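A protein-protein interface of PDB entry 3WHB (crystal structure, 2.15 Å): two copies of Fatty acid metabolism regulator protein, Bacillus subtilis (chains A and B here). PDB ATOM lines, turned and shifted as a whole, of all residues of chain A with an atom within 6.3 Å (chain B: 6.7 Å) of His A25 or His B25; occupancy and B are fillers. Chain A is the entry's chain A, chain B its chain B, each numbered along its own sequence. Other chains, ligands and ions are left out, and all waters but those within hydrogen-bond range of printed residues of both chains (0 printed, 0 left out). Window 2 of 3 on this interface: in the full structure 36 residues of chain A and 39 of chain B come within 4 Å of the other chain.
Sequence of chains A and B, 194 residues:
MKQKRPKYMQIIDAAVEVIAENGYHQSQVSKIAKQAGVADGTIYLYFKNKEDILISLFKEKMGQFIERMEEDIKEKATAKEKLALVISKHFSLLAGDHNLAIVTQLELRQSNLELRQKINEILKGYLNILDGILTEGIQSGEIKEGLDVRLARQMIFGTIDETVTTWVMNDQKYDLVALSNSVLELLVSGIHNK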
ATOM      1  N   ASN A  22      -9.686   2.159  -6.961  1.00  0.00           N
ATOM      2  CA  ASN A  22      -8.727   1.184  -7.474  1.00  0.00           C
ATOM      3  C   ASN A  22      -7.502   1.771  -8.158  1.00  0.00           C
ATOM      4  O   ASN A  22      -6.497   1.085  -8.332  1.00  0.00           O
ATOM      5  CB  ASN A  22      -9.429   0.233  -8.445  1.00  0.00           C
ATOM      6  CG  ASN A  22     -10.430  -0.660  -7.753  1.00  0.00           C
ATOM      7  OD1 ASN A  22     -10.074  -1.711  -7.226  1.00  0.00           O
ATOM      8  ND2 ASN A  22     -11.690  -0.246  -7.743  1.00  0.00           N
ATOM      9  N   GLY A  23      -7.581   3.040  -8.543  1.00  0.00           N
ATOM     10  CA  GLY A  23      -6.548   3.647  -9.378  1.00  0.00           C
ATOM     11  C   GLY A  23      -6.942   3.474 -10.829  1.00  0.00           C
ATOM     12  O   GLY A  23      -7.569   2.473 -11.190  1.00  0.00           O
ATOM     13  N   TYR A  24      -6.575   4.446 -11.659  1.00  0.00           N
ATOM     14  CA  TYR A  24      -6.978   4.469 -13.064  1.00  0.00           C
ATOM     15  C   TYR A  24      -6.496   3.261 -13.860  1.00  0.00           C
ATOM     16  O   TYR A  24      -7.244   2.704 -14.662  1.00  0.00           O
ATOM     17  CB  TYR A  24      -6.510   5.762 -13.741  1.00  0.00           C
ATOM     18  CG  TYR A  24      -6.620   5.739 -15.251  1.00  0.00           C
ATOM     19  CD1 TYR A  24      -7.852   5.902 -15.885  1.00  0.00           C
ATOM     20  CD2 TYR A  24      -5.488   5.550 -16.044  1.00  0.00           C
ATOM     21  CE1 TYR A  24      -7.952   5.880 -17.267  1.00  0.00           C
ATOM     22  CE2 TYR A  24      -5.578   5.532 -17.422  1.00  0.00           C
ATOM     23  CZ  TYR A  24      -6.811   5.698 -18.025  1.00  0.00           C
ATOM     24  OH  TYR A  24      -6.895   5.680 -19.393  1.00  0.00           O
ATOM     25  N   HIS A  25      -5.243   2.870 -13.649  1.00  0.00           N
ATOM     26  CA  HIS A  25      -4.668   1.747 -14.378  1.00  0.00           C
ATOM     27  C   HIS A  25      -5.251   0.417 -13.947  1.00  0.00           C
ATOM     28  O   HIS A  25      -5.479  -0.457 -14.778  1.00  0.00           O
ATOM     29  CB  HIS A  25      -3.149   1.748 -14.258  1.00  0.00           C
ATOM     30  CG  HIS A  25      -2.501   2.842 -15.039  1.00  0.00           C
ATOM     31  ND1 HIS A  25      -2.473   2.850 -16.418  1.00  0.00           N
ATOM     32  CD2 HIS A  25      -1.887   3.981 -14.643  1.00  0.00           C
ATOM     33  CE1 HIS A  25      -1.860   3.943 -16.836  1.00  0.00           C
ATOM     34  NE2 HIS A  25      -1.495   4.646 -15.778  1.00  0.00           N
ATOM     35  N   GLN A  26      -5.510   0.277 -12.652  1.00  0.00           N
ATOM     36  CA  GLN A  26      -6.142  -0.924 -12.128  1.00  0.00           C
ATOM     37  C   GLN A  26      -7.660  -0.907 -12.330  1.00  0.00           C
ATOM     38  O   GLN A  26      -8.327  -1.916 -12.115  1.00  0.00           O
ATOM     39  CB  GLN A  26      -5.775  -1.138 -10.654  1.00  0.00           C
ATOM     40  CG  GLN A  26      -4.336  -1.594 -10.425  1.00  0.00           C
ATOM     41  CD  GLN A  26      -4.095  -3.052 -10.797  1.00  0.00           C
ATOM     42  OE1 GLN A  26      -5.036  -3.826 -10.998  1.00  0.00           O
ATOM     43  NE2 GLN A  26      -2.822  -3.436 -10.885  1.00  0.00           N
ATOM     44  N   SER A  27      -8.201   0.239 -12.741  1.00  0.00           N
ATOM     45  CA  SER A  27      -9.607   0.330 -13.124  1.00  0.00           C
ATOM     46  C   SER A  27      -9.780  -0.319 -14.485  1.00  0.00           C
ATOM     47  O   SER A  27      -8.933  -0.149 -15.362  1.00  0.00           O
ATOM     48  CB  SER A  27     -10.061   1.784 -13.211  1.00  0.00           C
ATOM     49  OG  SER A  27      -9.954   2.428 -11.958  1.00  0.00           O
ATOM     50  N   GLN A  28     -10.862  -1.072 -14.656  1.00  0.00           N
ATOM     51  CA  GLN A  28     -11.212  -1.585 -15.980  1.00  0.00           C
ATOM     52  C   GLN A  28     -12.695  -1.402 -16.303  1.00  0.00           C
ATOM     53  O   GLN A  28     -13.541  -1.373 -15.406  1.00  0.00           O
ATOM     54  CB  GLN A  28     -10.762  -3.045 -16.154  1.00  0.00           C
ATOM     55  CG  GLN A  28     -10.568  -3.482 -17.608  1.00  0.00           C
ATOM     56  CD  GLN A  28      -9.728  -2.507 -18.431  1.00  0.00           C
ATOM     57  OE1 GLN A  28     -10.198  -1.959 -19.434  1.00  0.00           O
ATOM     58  NE2 GLN A  28      -8.482  -2.280 -18.006  1.00  0.00           N
ATOM     59  N   LYS A  50     -11.532   3.144 -21.934  1.00  0.00           N
ATOM     60  CA  LYS A  50     -11.275   3.628 -20.572  1.00  0.00           C
ATOM     61  C   LYS A  50     -10.683   5.042 -20.570  1.00  0.00           C
ATOM     62  O   LYS A  50     -11.074   5.893 -19.766  1.00  0.00           O
ATOM     63  CB  LYS A  50     -10.343   2.661 -19.834  1.00  0.00           C
ATOM     64  CG  LYS A  50     -10.110   3.000 -18.371  1.00  0.00           C
ATOM     65  CD  LYS A  50      -9.333   1.909 -17.651  1.00  0.00           C
ATOM     66  CE  LYS A  50      -7.834   1.969 -17.923  1.00  0.00           C
ATOM     67  NZ  LYS A  50      -7.118   0.901 -17.171  1.00  0.00           N
ATOM     68  N   GLU A 107      -5.492  10.487  -9.959  1.00  0.00           N
ATOM     69  CA  GLU A 107      -5.823   9.572 -11.047  1.00  0.00           C
ATOM     70  C   GLU A 107      -5.840  10.214 -12.436  1.00  0.00           C
ATOM     71  O   GLU A 107      -5.544   9.550 -13.423  1.00  0.00           O
ATOM     72  CB  GLU A 107      -7.136   8.845 -10.753  1.00  0.00           C
ATOM     73  CG  GLU A 107      -7.142   8.054  -9.441  1.00  0.00           C
ATOM     74  CD  GLU A 107      -5.922   7.160  -9.264  1.00  0.00           C
ATOM     75  OE1 GLU A 107      -5.432   6.581 -10.260  1.00  0.00           O
ATOM     76  OE2 GLU A 107      -5.452   7.031  -8.117  1.00  0.00           O
ATOM     77  N   GLN A 110      -2.026  11.489 -15.202  1.00  0.00           N
ATOM     78  CA  GLN A 110      -1.404  10.476 -16.048  1.00  0.00           C
ATOM     79  C   GLN A 110      -0.118  11.005 -16.657  1.00  0.00           C
ATOM     80  O   GLN A 110      -0.015  12.188 -16.998  1.00  0.00           O
ATOM     81  CB  GLN A 110      -2.365  10.019 -17.151  1.00  0.00           C
ATOM     82  CG  GLN A 110      -3.577   9.258 -16.634  1.00  0.00           C
ATOM     83  CD  GLN A 110      -3.204   8.099 -15.726  1.00  0.00           C
ATOM     84  OE1 GLN A 110      -2.455   7.200 -16.114  1.00  0.00           O
ATOM     85  NE2 GLN A 110      -3.727   8.116 -14.507  1.00  0.00           N
ATOM     86  N   SER A 111       0.861  10.116 -16.788  1.00  0.00           N
ATOM     87  CA  SER A 111       2.183  10.494 -17.259  1.00  0.00           C
ATOM     88  C   SER A 111       2.384  10.194 -18.736  1.00  0.00           C
ATOM     89  O   SER A 111       3.435  10.513 -19.298  1.00  0.00           O
ATOM     90  CB  SER A 111       3.260   9.807 -16.428  1.00  0.00           C
ATOM     91  OG  SER A 111       3.175   8.395 -16.531  1.00  0.00           O
ATOM     92  N   ILE B  19      11.184   6.117 -19.119  1.00  0.00           N
ATOM     93  CA  ILE B  19      10.011   6.567 -18.368  1.00  0.00           C
ATOM     94  C   ILE B  19       9.412   7.835 -18.977  1.00  0.00           C
ATOM     95  O   ILE B  19       8.191   7.965 -19.058  1.00  0.00           O
ATOM     96  CB  ILE B  19      10.337   6.756 -16.860  1.00  0.00           C
ATOM     97  CG1 ILE B  19      10.654   5.397 -16.218  1.00  0.00           C
ATOM     98  CG2 ILE B  19       9.192   7.454 -16.125  1.00  0.00           C
ATOM     99  CD1 ILE B  19      11.230   5.467 -14.818  1.00  0.00           C
ATOM    100  N   ASN B  22       7.177   7.051 -22.574  1.00  0.00           N
ATOM    101  CA  ASN B  22       5.805   6.525 -22.565  1.00  0.00           C
ATOM    102  C   ASN B  22       5.050   6.740 -21.252  1.00  0.00           C
ATOM    103  O   ASN B  22       3.838   6.522 -21.177  1.00  0.00           O
ATOM    104  CB  ASN B  22       5.807   5.029 -22.897  1.00  0.00           C
ATOM    105  CG  ASN B  22       6.735   4.684 -24.044  1.00  0.00           C
ATOM    106  OD1 ASN B  22       6.587   5.193 -25.159  1.00  0.00           O
ATOM    107  ND2 ASN B  22       7.698   3.805 -23.778  1.00  0.00           N
ATOM    108  N   GLY B  23       5.769   7.171 -20.224  1.00  0.00           N
ATOM    109  CA  GLY B  23       5.222   7.228 -18.880  1.00  0.00           C
ATOM    110  C   GLY B  23       5.702   6.006 -18.129  1.00  0.00           C
ATOM    111  O   GLY B  23       6.091   5.005 -18.742  1.00  0.00           O
ATOM    112  N   TYR B  24       5.670   6.093 -16.802  1.00  0.00           N
ATOM    113  CA  TYR B  24       6.208   5.058 -15.924  1.00  0.00           C
ATOM    114  C   TYR B  24       5.467   3.733 -16.053  1.00  0.00           C
ATOM    115  O   TYR B  24       6.096   2.677 -16.137  1.00  0.00           O
ATOM    116  CB  TYR B  24       6.203   5.533 -14.462  1.00  0.00           C
ATOM    117  CG  TYR B  24       6.389   4.422 -13.460  1.00  0.00           C
ATOM    118  CD1 TYR B  24       7.657   3.905 -13.188  1.00  0.00           C
ATOM    119  CD2 TYR B  24       5.293   3.870 -12.798  1.00  0.00           C
ATOM    120  CE1 TYR B  24       7.827   2.875 -12.275  1.00  0.00           C
ATOM    121  CE2 TYR B  24       5.455   2.844 -11.887  1.00  0.00           C
ATOM    122  CZ  TYR B  24       6.721   2.348 -11.627  1.00  0.00           C
ATOM    123  OH  TYR B  24       6.873   1.324 -10.721  1.00  0.00           O
ATOM    124  N   HIS B  25       4.138   3.795 -16.065  1.00  0.00           N
ATOM    125  CA  HIS B  25       3.299   2.597 -16.150  1.00  0.00           C
ATOM    126  C   HIS B  25       3.552   1.811 -17.442  1.00  0.00           C
ATOM    127  O   HIS B  25       3.649   0.587 -17.415  1.00  0.00           O
ATOM    128  CB  HIS B  25       1.818   2.969 -16.016  1.00  0.00           C
ATOM    129  CG  HIS B  25       0.898   1.789 -15.932  1.00  0.00           C
ATOM    130  ND1 HIS B  25       0.236   1.280 -17.030  1.00  0.00           N
ATOM    131  CD2 HIS B  25       0.524   1.022 -14.880  1.00  0.00           C
ATOM    132  CE1 HIS B  25      -0.503   0.249 -16.659  1.00  0.00           C
ATOM    133  NE2 HIS B  25      -0.347   0.071 -15.358  1.00  0.00           N
ATOM    134  N   GLN B  26       3.678   2.524 -18.559  1.00  0.00           N
ATOM    135  CA  GLN B  26       3.933   1.898 -19.859  1.00  0.00           C
ATOM    136  C   GLN B  26       5.383   1.452 -20.053  1.00  0.00           C
ATOM    137  O   GLN B  26       5.652   0.529 -20.826  1.00  0.00           O
ATOM    138  CB  GLN B  26       3.542   2.842 -20.993  1.00  0.00           C
ATOM    139  CG  GLN B  26       2.046   2.939 -21.246  1.00  0.00           C
ATOM    140  CD  GLN B  26       1.703   3.966 -22.311  1.00  0.00           C
ATOM    141  OE1 GLN B  26       2.489   4.217 -23.231  1.00  0.00           O
ATOM    142  NE2 GLN B  26       0.523   4.565 -22.191  1.00  0.00           N
ATOM    143  N   SER B  27       6.312   2.116 -19.363  1.00  0.00           N
ATOM    144  CA  SER B  27       7.740   1.802 -19.477  1.00  0.00           C
ATOM    145  C   SER B  27       8.016   0.349 -19.105  1.00  0.00           C
ATOM    146  O   SER B  27       7.353  -0.208 -18.236  1.00  0.00           O
ATOM    147  CB  SER B  27       8.583   2.743 -18.608  1.00  0.00           C
ATOM    148  OG  SER B  27       8.462   2.432 -17.229  1.00  0.00           O
ATOM    149  N   GLN B  28       8.988  -0.258 -19.780  1.00  0.00           N
ATOM    150  CA  GLN B  28       9.370  -1.645 -19.515  1.00  0.00           C
ATOM    151  C   GLN B  28      10.818  -1.764 -19.059  1.00  0.00           C
ATOM    152  O   GLN B  28      11.699  -1.066 -19.571  1.00  0.00           O
ATOM    153  CB  GLN B  28       9.162  -2.506 -20.757  1.00  0.00           C
ATOM    154  CG  GLN B  28       7.711  -2.771 -21.114  1.00  0.00           C
ATOM    155  CD  GLN B  28       7.585  -3.612 -22.365  1.00  0.00           C
ATOM    156  OE1 GLN B  28       8.350  -4.558 -22.566  1.00  0.00           O
ATOM    157  NE2 GLN B  28       6.624  -3.272 -23.215  1.00  0.00           N
ATOM    158  N   LYS B  50      10.866  -2.642 -10.839  1.00  0.00           N
ATOM    159  CA  LYS B  50      10.545  -1.430 -11.588  1.00  0.00           C
ATOM    160  C   LYS B  50      10.298  -0.244 -10.656  1.00  0.00           C
ATOM    161  O   LYS B  50      10.737   0.884 -10.921  1.00  0.00           O
ATOM    162  CB  LYS B  50       9.300  -1.694 -12.433  1.00  0.00           C
ATOM    163  CG  LYS B  50       9.003  -0.648 -13.488  1.00  0.00           C
ATOM    164  CD  LYS B  50       7.536  -0.720 -13.855  1.00  0.00           C
ATOM    165  CE  LYS B  50       7.270   0.010 -15.150  1.00  0.00           C
ATOM    166  NZ  LYS B  50       5.811   0.110 -15.412  1.00  0.00           N
ATOM    167  N   GLU B 107       5.514  12.211 -12.824  1.00  0.00           N
ATOM    168  CA  GLU B 107       5.568  11.011 -11.977  1.00  0.00           C
ATOM    169  C   GLU B 107       5.752  11.321 -10.492  1.00  0.00           C
ATOM    170  O   GLU B 107       5.997  10.417  -9.688  1.00  0.00           O
ATOM    171  CB  GLU B 107       6.662  10.051 -12.453  1.00  0.00           C
ATOM    172  CG  GLU B 107       6.696   9.814 -13.954  1.00  0.00           C
ATOM    173  CD  GLU B 107       5.609   8.879 -14.452  1.00  0.00           C
ATOM    174  OE1 GLU B 107       4.735   8.448 -13.663  1.00  0.00           O
ATOM    175  OE2 GLU B 107       5.633   8.568 -15.660  1.00  0.00           O
ATOM    176  N   SER B 111      -0.257   7.091  -7.838  1.00  0.00           N
ATOM    177  CA  SER B 111      -1.523   6.526  -7.385  1.00  0.00           C
ATOM    178  C   SER B 111      -1.311   5.479  -6.289  1.00  0.00           C
ATOM    179  O   SER B 111      -1.979   5.512  -5.253  1.00  0.00           O
ATOM    180  CB  SER B 111      -2.280   5.915  -8.564  1.00  0.00           C
ATOM    181  OG  SER B 111      -3.461   5.272  -8.128  1.00  0.00           O
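Of the 11 printed residues of chain A, 4 touch a printed residue of chain B. Hydrophobic or aromatic side chains of chain A within 4 Å of the printed part of chain B: His A25. Among the printed residues, no Asp or Glu carboxylate lies within 4 Å of a Lys or Arg side-chain nitrogen of the other chain.
O of Tyr B24 is in hydrogen-bond range of NZ of Lys B50 (2.7 Å). NE2 of Gln A110 is in hydrogen-bond range of O of Glu A107 (2.6 Å). O of Gly A23 lies within hydrogen-bond range of OG of Ser A27. O of His A25 lies within hydrogen-bond range of NZ of Lys A50. O of Tyr B24 lies within hydrogen-bond range of OG of Ser B27 (2.6 Å). The backbone NH of Tyr A24 sits at hydrogen-bond distance from the side-chain carboxylate of Glu A107 (2.8 Å).
The side-chain hydroxyl of Ser A111 sits at hydrogen-bond distance from the backbone NH of Tyr B24. OE2 of Glu A107 lies within hydrogen-bond range of OG of Ser B111, at 2.7 Å. ND1 of His A25 is in hydrogen-bond range of ND1 of His B25 (3.2 Å). The side-chain hydroxyl of Ser A111 is in hydrogen-bond range of the side-chain carboxylate of Glu B107, 2.6 Å away.
Gly A23 touches Ser B111, and with the chains exchanged Ser A111 touches Gly B23. His A25 touches its own counterpart, His B25. Glu A107 touches Ser B111, and with the chains exchanged Ser A111 touches Glu B107. Ser A111 touches Tyr B24, but with the chains exchanged Tyr A24 does not touch Ser B111 (4.8 Å). Positions printed for both chains: 22, 23, 24, 25, 26, 27, 28, 50, 107 and 111. Of the 6 pairs that touch across the chains among the printed residues, 5 have their exchanged pair printed and touching as well.
Among the printed residues, pairs that only touch across the chains: Ser A111 with Gly B23 and Gly A23 with Ser B111.
Of chain B, only His B25 comes within 4 Å of His A25. Of the printed residues of chain B, Ser A111 touches Gly B23, Tyr B24 and Glu B107. Printed residues of chain A within 4 Å of Gly B23: Ser A111 (3.3 Å). Of the printed residues of chain A, Tyr B24 touches Ser A111 (3.4 Å). His B25 touches one residue of chain A. Of the printed residues of chain A, Glu B107 touches Ser A111. Of the printed residues of chain A, Ser B111 touches Gly A23 (3.7 Å) and Glu A107 (2.7 Å). The nearest printed residue of chain A that does not touch Glu B107 is Gln A110 (6.2 Å).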
